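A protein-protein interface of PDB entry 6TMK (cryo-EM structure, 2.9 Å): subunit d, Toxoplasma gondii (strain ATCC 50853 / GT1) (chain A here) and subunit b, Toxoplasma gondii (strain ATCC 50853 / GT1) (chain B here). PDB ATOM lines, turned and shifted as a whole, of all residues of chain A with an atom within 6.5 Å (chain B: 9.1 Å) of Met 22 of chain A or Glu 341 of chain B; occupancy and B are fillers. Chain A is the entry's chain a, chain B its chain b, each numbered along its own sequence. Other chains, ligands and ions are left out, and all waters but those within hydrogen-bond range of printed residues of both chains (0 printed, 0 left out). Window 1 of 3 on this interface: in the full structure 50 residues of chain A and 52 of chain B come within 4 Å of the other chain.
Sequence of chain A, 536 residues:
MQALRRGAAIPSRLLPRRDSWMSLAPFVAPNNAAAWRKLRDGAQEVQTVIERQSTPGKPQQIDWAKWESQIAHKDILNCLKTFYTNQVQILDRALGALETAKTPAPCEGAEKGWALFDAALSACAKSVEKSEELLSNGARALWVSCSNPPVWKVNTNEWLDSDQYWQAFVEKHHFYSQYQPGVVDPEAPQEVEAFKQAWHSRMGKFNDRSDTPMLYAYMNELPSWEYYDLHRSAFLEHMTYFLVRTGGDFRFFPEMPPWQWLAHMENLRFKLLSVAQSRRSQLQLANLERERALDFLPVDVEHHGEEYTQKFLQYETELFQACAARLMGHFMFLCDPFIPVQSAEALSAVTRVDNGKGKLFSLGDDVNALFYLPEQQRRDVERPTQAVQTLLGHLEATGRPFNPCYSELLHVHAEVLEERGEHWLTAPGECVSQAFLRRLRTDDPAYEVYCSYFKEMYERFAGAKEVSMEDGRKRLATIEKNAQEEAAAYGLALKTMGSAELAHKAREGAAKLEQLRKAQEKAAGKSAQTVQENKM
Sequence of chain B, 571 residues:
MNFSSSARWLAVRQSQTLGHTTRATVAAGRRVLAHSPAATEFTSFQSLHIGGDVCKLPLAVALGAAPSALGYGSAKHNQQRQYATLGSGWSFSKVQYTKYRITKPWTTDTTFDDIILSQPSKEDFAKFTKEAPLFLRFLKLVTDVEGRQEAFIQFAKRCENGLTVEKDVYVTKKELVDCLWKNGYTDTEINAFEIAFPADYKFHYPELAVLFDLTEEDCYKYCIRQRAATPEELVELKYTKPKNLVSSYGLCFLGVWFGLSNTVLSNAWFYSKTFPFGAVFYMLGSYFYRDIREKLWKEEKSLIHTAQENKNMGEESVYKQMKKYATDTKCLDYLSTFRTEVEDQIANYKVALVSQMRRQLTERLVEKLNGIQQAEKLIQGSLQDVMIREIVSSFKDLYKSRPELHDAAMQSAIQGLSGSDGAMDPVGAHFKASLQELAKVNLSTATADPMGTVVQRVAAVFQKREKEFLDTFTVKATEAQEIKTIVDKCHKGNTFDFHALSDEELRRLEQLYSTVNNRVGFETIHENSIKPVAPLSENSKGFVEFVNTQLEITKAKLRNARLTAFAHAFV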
ATOM      1  N   SER A  20     -11.728  25.130  -3.481  1.00  0.00           N
ATOM      2  CA  SER A  20     -12.701  24.659  -2.505  1.00  0.00           C
ATOM      3  C   SER A  20     -12.708  25.560  -1.276  1.00  0.00           C
ATOM      4  O   SER A  20     -13.699  25.626  -0.549  1.00  0.00           O
ATOM      5  CB  SER A  20     -12.396  23.217  -2.100  1.00  0.00           C
ATOM      6  OG  SER A  20     -13.524  22.604  -1.502  1.00  0.00           O
ATOM      7  N   TRP A  21     -11.596  26.259  -1.050  1.00  0.00           N
ATOM      8  CA  TRP A  21     -11.419  27.053   0.160  1.00  0.00           C
ATOM      9  C   TRP A  21     -12.374  28.234   0.242  1.00  0.00           C
ATOM     10  O   TRP A  21     -12.371  28.936   1.260  1.00  0.00           O
ATOM     11  CB  TRP A  21      -9.979  27.554   0.255  1.00  0.00           C
ATOM     12  CG  TRP A  21      -9.600  28.496  -0.833  1.00  0.00           C
ATOM     13  CD1 TRP A  21      -9.008  28.184  -2.020  1.00  0.00           C
ATOM     14  CD2 TRP A  21      -9.781  29.914  -0.835  1.00  0.00           C
ATOM     15  NE1 TRP A  21      -8.814  29.321  -2.765  1.00  0.00           N
ATOM     16  CE2 TRP A  21      -9.278  30.398  -2.057  1.00  0.00           C
ATOM     17  CE3 TRP A  21     -10.320  30.823   0.077  1.00  0.00           C
ATOM     18  CZ2 TRP A  21      -9.301  31.748  -2.390  1.00  0.00           C
ATOM     19  CZ3 TRP A  21     -10.342  32.162  -0.255  1.00  0.00           C
ATOM     20  CH2 TRP A  21      -9.836  32.613  -1.477  1.00  0.00           C
ATOM     21  N   MET A  22     -13.181  28.477  -0.790  1.00  0.00           N
ATOM     22  CA  MET A  22     -14.134  29.577  -0.758  1.00  0.00           C
ATOM     23  C   MET A  22     -15.389  29.231   0.029  1.00  0.00           C
ATOM     24  O   MET A  22     -16.134  30.140   0.411  1.00  0.00           O
ATOM     25  CB  MET A  22     -14.520  29.970  -2.184  1.00  0.00           C
ATOM     26  CG  MET A  22     -13.441  30.734  -2.925  1.00  0.00           C
ATOM     27  SD  MET A  22     -12.144  29.645  -3.541  1.00  0.00           S
ATOM     28  CE  MET A  22     -12.872  29.095  -5.080  1.00  0.00           C
ATOM     29  N   SER A  23     -15.632  27.948   0.282  1.00  0.00           N
ATOM     30  CA  SER A  23     -16.744  27.501   1.107  1.00  0.00           C
ATOM     31  C   SER A  23     -16.369  27.414   2.580  1.00  0.00           C
ATOM     32  O   SER A  23     -16.990  26.651   3.328  1.00  0.00           O
ATOM     33  CB  SER A  23     -17.252  26.147   0.610  1.00  0.00           C
ATOM     34  OG  SER A  23     -16.499  25.086   1.163  1.00  0.00           O
ATOM     35  N   LEU A  24     -15.366  28.177   3.006  1.00  0.00           N
ATOM     36  CA  LEU A  24     -14.892  28.189   4.382  1.00  0.00           C
ATOM     37  C   LEU A  24     -15.557  29.283   5.212  1.00  0.00           C
ATOM     38  O   LEU A  24     -15.034  29.662   6.265  1.00  0.00           O
ATOM     39  CB  LEU A  24     -13.372  28.358   4.389  1.00  0.00           C
ATOM     40  CG  LEU A  24     -12.604  28.363   5.707  1.00  0.00           C
ATOM     41  CD1 LEU A  24     -13.094  27.263   6.612  1.00  0.00           C
ATOM     42  CD2 LEU A  24     -11.122  28.211   5.435  1.00  0.00           C
ATOM     43  N   ALA A  25     -16.711  29.788   4.760  1.00  0.00           N
ATOM     44  CA  ALA A  25     -17.336  30.921   5.445  1.00  0.00           C
ATOM     45  C   ALA A  25     -17.843  30.547   6.831  1.00  0.00           C
ATOM     46  O   ALA A  25     -17.405  31.160   7.819  1.00  0.00           O
ATOM     47  CB  ALA A  25     -18.455  31.496   4.578  1.00  0.00           C
ATOM     48  N   TRP A  36     -11.570  38.132   6.876  1.00  0.00           N
ATOM     49  CA  TRP A  36     -12.146  37.228   5.886  1.00  0.00           C
ATOM     50  C   TRP A  36     -12.738  37.997   4.713  1.00  0.00           C
ATOM     51  O   TRP A  36     -12.519  37.645   3.550  1.00  0.00           O
ATOM     52  CB  TRP A  36     -13.207  36.348   6.546  1.00  0.00           C
ATOM     53  CG  TRP A  36     -14.189  35.784   5.580  1.00  0.00           C
ATOM     54  CD1 TRP A  36     -15.449  36.237   5.333  1.00  0.00           C
ATOM     55  CD2 TRP A  36     -13.992  34.656   4.724  1.00  0.00           C
ATOM     56  NE1 TRP A  36     -16.050  35.461   4.374  1.00  0.00           N
ATOM     57  CE2 TRP A  36     -15.176  34.482   3.985  1.00  0.00           C
ATOM     58  CE3 TRP A  36     -12.930  33.776   4.512  1.00  0.00           C
ATOM     59  CZ2 TRP A  36     -15.326  33.464   3.050  1.00  0.00           C
ATOM     60  CZ3 TRP A  36     -13.080  32.768   3.585  1.00  0.00           C
ATOM     61  CH2 TRP A  36     -14.268  32.619   2.865  1.00  0.00           C
ATOM     62  N   ARG A  40     -11.770  37.877   0.786  1.00  0.00           N
ATOM     63  CA  ARG A  40     -12.792  37.567  -0.204  1.00  0.00           C
ATOM     64  C   ARG A  40     -12.809  38.615  -1.306  1.00  0.00           C
ATOM     65  O   ARG A  40     -12.807  38.284  -2.496  1.00  0.00           O
ATOM     66  CB  ARG A  40     -14.156  37.474   0.483  1.00  0.00           C
ATOM     67  CG  ARG A  40     -15.351  37.422  -0.457  1.00  0.00           C
ATOM     68  CD  ARG A  40     -15.304  36.192  -1.342  1.00  0.00           C
ATOM     69  NE  ARG A  40     -15.436  34.961  -0.570  1.00  0.00           N
ATOM     70  CZ  ARG A  40     -15.309  33.739  -1.080  1.00  0.00           C
ATOM     71  NH1 ARG A  40     -15.047  33.575  -2.369  1.00  0.00           N
ATOM     72  NH2 ARG A  40     -15.446  32.679  -0.296  1.00  0.00           N
ATOM     73  N   ALA A  43      -9.854  38.348  -3.673  1.00  0.00           N
ATOM     74  CA  ALA A  43     -10.025  37.305  -4.679  1.00  0.00           C
ATOM     75  C   ALA A  43     -11.058  37.722  -5.717  1.00  0.00           C
ATOM     76  O   ALA A  43     -10.919  37.413  -6.907  1.00  0.00           O
ATOM     77  CB  ALA A  43     -10.432  35.994  -4.012  1.00  0.00           C
ATOM     78  N   ASP B 333      -9.417  20.269   5.321  1.00  0.00           N
ATOM     79  CA  ASP B 333      -9.109  19.923   3.939  1.00  0.00           C
ATOM     80  C   ASP B 333      -9.557  20.979   2.941  1.00  0.00           C
ATOM     81  O   ASP B 333      -9.173  20.896   1.770  1.00  0.00           O
ATOM     82  CB  ASP B 333      -9.753  18.582   3.587  1.00  0.00           C
ATOM     83  CG  ASP B 333     -11.210  18.720   3.195  1.00  0.00           C
ATOM     84  OD1 ASP B 333     -11.907  19.579   3.774  1.00  0.00           O
ATOM     85  OD2 ASP B 333     -11.661  17.965   2.308  1.00  0.00           O
ATOM     86  N   TYR B 334     -10.356  21.960   3.361  1.00  0.00           N
ATOM     87  CA  TYR B 334     -10.478  23.185   2.579  1.00  0.00           C
ATOM     88  C   TYR B 334      -9.202  24.011   2.650  1.00  0.00           C
ATOM     89  O   TYR B 334      -8.750  24.561   1.640  1.00  0.00           O
ATOM     90  CB  TYR B 334     -11.665  24.007   3.076  1.00  0.00           C
ATOM     91  CG  TYR B 334     -13.021  23.398   2.802  1.00  0.00           C
ATOM     92  CD1 TYR B 334     -13.176  22.365   1.891  1.00  0.00           C
ATOM     93  CD2 TYR B 334     -14.147  23.860   3.462  1.00  0.00           C
ATOM     94  CE1 TYR B 334     -14.413  21.809   1.647  1.00  0.00           C
ATOM     95  CE2 TYR B 334     -15.386  23.309   3.227  1.00  0.00           C
ATOM     96  CZ  TYR B 334     -15.515  22.288   2.316  1.00  0.00           C
ATOM     97  OH  TYR B 334     -16.753  21.740   2.077  1.00  0.00           O
ATOM     98  N   LEU B 335      -8.611  24.110   3.842  1.00  0.00           N
ATOM     99  CA  LEU B 335      -7.415  24.925   4.026  1.00  0.00           C
ATOM    100  C   LEU B 335      -6.279  24.480   3.113  1.00  0.00           C
ATOM    101  O   LEU B 335      -5.501  25.311   2.630  1.00  0.00           O
ATOM    102  CB  LEU B 335      -6.973  24.867   5.485  1.00  0.00           C
ATOM    103  CG  LEU B 335      -6.206  26.068   6.037  1.00  0.00           C
ATOM    104  CD1 LEU B 335      -6.998  27.350   5.880  1.00  0.00           C
ATOM    105  CD2 LEU B 335      -5.863  25.839   7.489  1.00  0.00           C
ATOM    106  N   SER B 336      -6.162  23.174   2.866  1.00  0.00           N
ATOM    107  CA  SER B 336      -5.079  22.681   2.021  1.00  0.00           C
ATOM    108  C   SER B 336      -5.173  23.243   0.607  1.00  0.00           C
ATOM    109  O   SER B 336      -4.151  23.580  -0.003  1.00  0.00           O
ATOM    110  CB  SER B 336      -5.105  21.154   1.991  1.00  0.00           C
ATOM    111  OG  SER B 336      -5.311  20.626   3.289  1.00  0.00           O
ATOM    112  N   THR B 337      -6.388  23.354   0.071  1.00  0.00           N
ATOM    113  CA  THR B 337      -6.550  23.832  -1.299  1.00  0.00           C
ATOM    114  C   THR B 337      -6.013  25.249  -1.453  1.00  0.00           C
ATOM    115  O   THR B 337      -5.462  25.605  -2.502  1.00  0.00           O
ATOM    116  CB  THR B 337      -8.021  23.772  -1.720  1.00  0.00           C
ATOM    117  OG1 THR B 337      -8.715  24.922  -1.219  1.00  0.00           O
ATOM    118  CG2 THR B 337      -8.691  22.502  -1.210  1.00  0.00           C
ATOM    119  N   PHE B 338      -6.181  26.073  -0.419  1.00  0.00           N
ATOM    120  CA  PHE B 338      -5.738  27.464  -0.445  1.00  0.00           C
ATOM    121  C   PHE B 338      -4.345  27.639  -1.042  1.00  0.00           C
ATOM    122  O   PHE B 338      -4.153  28.421  -1.978  1.00  0.00           O
ATOM    123  CB  PHE B 338      -5.780  28.012   0.981  1.00  0.00           C
ATOM    124  CG  PHE B 338      -5.648  29.500   1.066  1.00  0.00           C
ATOM    125  CD1 PHE B 338      -6.740  30.318   0.844  1.00  0.00           C
ATOM    126  CD2 PHE B 338      -4.439  30.079   1.397  1.00  0.00           C
ATOM    127  CE1 PHE B 338      -6.625  31.688   0.932  1.00  0.00           C
ATOM    128  CE2 PHE B 338      -4.316  31.449   1.489  1.00  0.00           C
ATOM    129  CZ  PHE B 338      -5.411  32.255   1.257  1.00  0.00           C
ATOM    130  N   ARG B 339      -3.357  26.915  -0.514  1.00  0.00           N
ATOM    131  CA  ARG B 339      -2.001  27.033  -1.042  1.00  0.00           C
ATOM    132  C   ARG B 339      -1.902  26.540  -2.479  1.00  0.00           C
ATOM    133  O   ARG B 339      -1.129  27.091  -3.270  1.00  0.00           O
ATOM    134  CB  ARG B 339      -1.029  26.259  -0.152  1.00  0.00           C
ATOM    135  CG  ARG B 339       0.391  26.172  -0.690  1.00  0.00           C
ATOM    136  CD  ARG B 339       1.004  27.548  -0.866  1.00  0.00           C
ATOM    137  NE  ARG B 339       2.396  27.479  -1.297  1.00  0.00           N
ATOM    138  CZ  ARG B 339       3.400  27.078  -0.523  1.00  0.00           C
ATOM    139  NH1 ARG B 339       4.636  27.050  -0.999  1.00  0.00           N
ATOM    140  NH2 ARG B 339       3.173  26.718   0.732  1.00  0.00           N
ATOM    141  N   THR B 340      -2.671  25.513  -2.833  1.00  0.00           N
ATOM    142  CA  THR B 340      -2.619  24.973  -4.189  1.00  0.00           C
ATOM    143  C   THR B 340      -3.266  25.914  -5.196  1.00  0.00           C
ATOM    144  O   THR B 340      -2.811  26.015  -6.341  1.00  0.00           O
ATOM    145  CB  THR B 340      -3.298  23.604  -4.230  1.00  0.00           C
ATOM    146  OG1 THR B 340      -2.522  22.660  -3.481  1.00  0.00           O
ATOM    147  CG2 THR B 340      -3.441  23.121  -5.665  1.00  0.00           C
ATOM    148  N   GLU B 341      -4.328  26.611  -4.792  1.00  0.00           N
ATOM    149  CA  GLU B 341      -5.084  27.439  -5.727  1.00  0.00           C
ATOM    150  C   GLU B 341      -4.395  28.772  -5.995  1.00  0.00           C
ATOM    151  O   GLU B 341      -4.198  29.151  -7.153  1.00  0.00           O
ATOM    152  CB  GLU B 341      -6.495  27.667  -5.189  1.00  0.00           C
ATOM    153  CG  GLU B 341      -7.422  26.480  -5.380  1.00  0.00           C
ATOM    154  CD  GLU B 341      -8.846  26.776  -4.957  1.00  0.00           C
ATOM    155  OE1 GLU B 341      -9.264  27.948  -5.048  1.00  0.00           O
ATOM    156  OE2 GLU B 341      -9.547  25.834  -4.531  1.00  0.00           O
ATOM    157  N   VAL B 342      -4.047  29.509  -4.940  1.00  0.00           N
ATOM    158  CA  VAL B 342      -3.583  30.884  -5.110  1.00  0.00           C
ATOM    159  C   VAL B 342      -2.286  30.942  -5.910  1.00  0.00           C
ATOM    160  O   VAL B 342      -2.057  31.898  -6.668  1.00  0.00           O
ATOM    161  CB  VAL B 342      -3.423  31.542  -3.726  1.00  0.00           C
ATOM    162  CG1 VAL B 342      -2.485  32.734  -3.794  1.00  0.00           C
ATOM    163  CG2 VAL B 342      -4.776  31.951  -3.187  1.00  0.00           C
ATOM    164  N   GLU B 343      -1.503  29.864  -5.882  1.00  0.00           N
ATOM    165  CA  GLU B 343      -0.292  29.729  -6.684  1.00  0.00           C
ATOM    166  C   GLU B 343      -0.578  29.340  -8.125  1.00  0.00           C
ATOM    167  O   GLU B 343       0.344  28.964  -8.856  1.00  0.00           O
ATOM    168  CB  GLU B 343       0.638  28.694  -6.047  1.00  0.00           C
ATOM    169  CG  GLU B 343       1.224  29.134  -4.718  1.00  0.00           C
ATOM    170  CD  GLU B 343       2.566  29.818  -4.870  1.00  0.00           C
ATOM    171  OE1 GLU B 343       2.854  30.326  -5.974  1.00  0.00           O
ATOM    172  OE2 GLU B 343       3.334  29.849  -3.885  1.00  0.00           O
ATOM    173  N   ASP B 344      -1.818  29.419  -8.526  1.00  0.00           N
ATOM    174  CA  ASP B 344      -2.282  29.259  -9.896  1.00  0.00           C
ATOM    175  C   ASP B 344      -3.129  30.448 -10.312  1.00  0.00           C
ATOM    176  O   ASP B 344      -3.021  30.914 -11.445  1.00  0.00           O
ATOM    177  CB  ASP B 344      -3.084  27.962 -10.039  1.00  0.00           C
ATOM    178  CG  ASP B 344      -3.176  27.490 -11.474  1.00  0.00           C
ATOM    179  OD1 ASP B 344      -2.169  26.967 -11.994  1.00  0.00           O
ATOM    180  OD2 ASP B 344      -4.256  27.642 -12.083  1.00  0.00           O
ATOM    181  N   GLN B 345      -3.998  30.921  -9.419  1.00  0.00           N
ATOM    182  CA  GLN B 345      -4.723  32.170  -9.622  1.00  0.00           C
ATOM    183  C   GLN B 345      -3.789  33.369  -9.768  1.00  0.00           C
ATOM    184  O   GLN B 345      -4.113  34.309 -10.505  1.00  0.00           O
ATOM    185  CB  GLN B 345      -5.692  32.394  -8.460  1.00  0.00           C
ATOM    186  CG  GLN B 345      -6.297  33.788  -8.403  1.00  0.00           C
ATOM    187  CD  GLN B 345      -7.422  33.933  -7.379  1.00  0.00           C
ATOM    188  OE1 GLN B 345      -7.893  35.041  -7.128  1.00  0.00           O
ATOM    189  NE2 GLN B 345      -7.855  32.823  -6.787  1.00  0.00           N
ATOM    190  N   ILE B 346      -2.555  33.279  -9.277  1.00  0.00           N
ATOM    191  CA  ILE B 346      -1.639  34.392  -9.506  1.00  0.00           C
ATOM    192  C   ILE B 346      -0.989  34.278 -10.879  1.00  0.00           C
ATOM    193  O   ILE B 346      -0.797  35.286 -11.577  1.00  0.00           O
ATOM    194  CB  ILE B 346      -0.589  34.434  -8.380  1.00  0.00           C
ATOM    195  CG1 ILE B 346      -1.213  34.945  -7.078  1.00  0.00           C
ATOM    196  CG2 ILE B 346       0.592  35.298  -8.779  1.00  0.00           C
ATOM    197  CD1 ILE B 346      -1.683  36.384  -7.124  1.00  0.00           C
ATOM    198  N   ALA B 347      -0.609  33.066 -11.279  1.00  0.00           N
ATOM    199  CA  ALA B 347      -0.072  32.897 -12.619  1.00  0.00           C
ATOM    200  C   ALA B 347      -1.133  33.169 -13.680  1.00  0.00           C
ATOM    201  O   ALA B 347      -0.798  33.587 -14.794  1.00  0.00           O
ATOM    202  CB  ALA B 347       0.494  31.488 -12.780  1.00  0.00           C
ATOM    203  N   ASN B 348      -2.413  32.944 -13.361  1.00  0.00           N
ATOM    204  CA  ASN B 348      -3.519  33.373 -14.209  1.00  0.00           C
ATOM    205  C   ASN B 348      -4.109  34.715 -13.783  1.00  0.00           C
ATOM    206  O   ASN B 348      -5.279  34.998 -14.059  1.00  0.00           O
ATOM    207  CB  ASN B 348      -4.607  32.301 -14.226  1.00  0.00           C
ATOM    208  CG  ASN B 348      -4.112  30.980 -14.775  1.00  0.00           C
ATOM    209  OD1 ASN B 348      -2.973  30.871 -15.228  1.00  0.00           O
ATOM    210  ND2 ASN B 348      -4.967  29.966 -14.737  1.00  0.00           N
ATOM    211  N   TYR B 349      -3.320  35.538 -13.113  1.00  0.00           N
ATOM    212  CA  TYR B 349      -3.631  36.935 -12.832  1.00  0.00           C
ATOM    213  C   TYR B 349      -2.643  37.871 -13.503  1.00  0.00           C
ATOM    214  O   TYR B 349      -3.039  38.915 -14.037  1.00  0.00           O
ATOM    215  CB  TYR B 349      -3.631  37.199 -11.325  1.00  0.00           C
ATOM    216  CG  TYR B 349      -3.986  38.621 -10.964  1.00  0.00           C
ATOM    217  CD1 TYR B 349      -3.142  39.386 -10.173  1.00  0.00           C
ATOM    218  CD2 TYR B 349      -5.158  39.201 -11.424  1.00  0.00           C
ATOM    219  CE1 TYR B 349      -3.460  40.685  -9.841  1.00  0.00           C
ATOM    220  CE2 TYR B 349      -5.485  40.501 -11.099  1.00  0.00           C
ATOM    221  CZ  TYR B 349      -4.632  41.240 -10.308  1.00  0.00           C
ATOM    222  OH  TYR B 349      -4.949  42.537  -9.982  1.00  0.00           O
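Hydrophobic or aromatic side chains of chain A that line the printed part of chain B: Trp 21 and Met 22.
Along chain A the printed residues that touch a printed residue of chain B span positions 20 to 43.
Printed residues of chain B that touch a printed residue of chain A: Tyr 334, Thr 337, Phe 338, Glu 341 and Gln 345.
Hydrophobic or aromatic side chains of chain B that line the printed part of chain A: Tyr 334 and Phe 338.
Among the printed residues, 10 pairs touch across the chains.
The side-chain hydroxyl (OH) of Tyr 334 of chain B lies close to the side-chain hydroxyl (OG) of Ser 23 of chain A, at 3.5 Å.
The side-chain carboxylate (OE2) of Glu 341 of chain B lies within hydrogen-bond range of the backbone NH (N) of Ser 20 of chain A (2.5 Å).
The side-chain carboxylate of Glu 341 of chain B is in hydrogen-bond range of the indole nitrogen of Trp 21 of chain A (2.7 Å).
SD of Met 22 of chain A sits close to OE1 of Glu 341 of chain B, 3.7 Å away.
OG1 of Thr 337 of chain B lies within hydrogen-bond range of N of Trp 21 of chain A (3.2 Å).
Of the printed residues of chain B, Ser 20 of chain A touches Tyr 334 (3.4 Å), Thr 337 (3.8 Å) and Glu 341 (2.5 Å).
Printed residues of chain B within 4 Å of Trp 21 of chain A: Tyr 334, Thr 337, Phe 338 and Glu 341.
Ser 23 of chain A touches just one residue of chain B: Tyr 334.
Printed residues of chain B within 4 Å of Ala 43 of chain A: Gln 345 (3.9 Å).
Of the printed residues of chain A, Tyr 334 of chain B touches Ser 20 (3.4 Å), Trp 21 (3.5 Å) and Ser 23 (2.9 Å).
Of the printed residues of chain A, Thr 337 of chain B touches Ser 20 and Trp 21.
Of the printed residues of chain A, Phe 338 of chain B touches Trp 21.
Thr 340 of chain B touches none of the printed residues of chain A.
Glu 341 of chain B touches just these residues of chain A: Ser 20 (2.5 Å), Trp 21 (2.7 Å) and Met 22 (3.7 Å).
Tyr 349 of chain B touches none of the printed residues of chain A.
The nearest residue of chain B that does not touch Met 22 of chain A is Thr 337 of chain B (5.7 Å).
The nearest printed residue of chain A that does not touch Phe 338 of chain B is Ser 20 of chain A (6.4 Å).
Ser 20 of chain A touches Tyr 334 of chain B (OG to CE1, 3.4 Å).
N of Ser 20 of chain A touches OG1 of Thr 337 of chain B (3.8 Å).
O of Tyr 334 of chain B touches CB of Trp 21 of chain A, at 3.5 Å.
Trp 21 of chain A touches Phe 338 of chain B (CD2 to CD1, 3.5 Å).
Ala 43 of chain A touches Gln 345 of chain B (O to OE1, 3.9 Å).
O of Met 22 of chain A sits at hydrogen-bond distance from NH2 of Arg 40 of chain A.
The backbone carbonyl oxygen of Ser 20 of chain A is in hydrogen-bond range of the side-chain hydroxyl of Ser 23 of chain A.
The side-chain sulfur of Met 22 of chain A lies close to the indole nitrogen of Trp 21 of chain A (3.4 Å).
The side-chain hydroxyl of Thr 337 of chain B is in hydrogen-bond range of the backbone carbonyl oxygen of Tyr 334 of chain B (2.9 Å).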
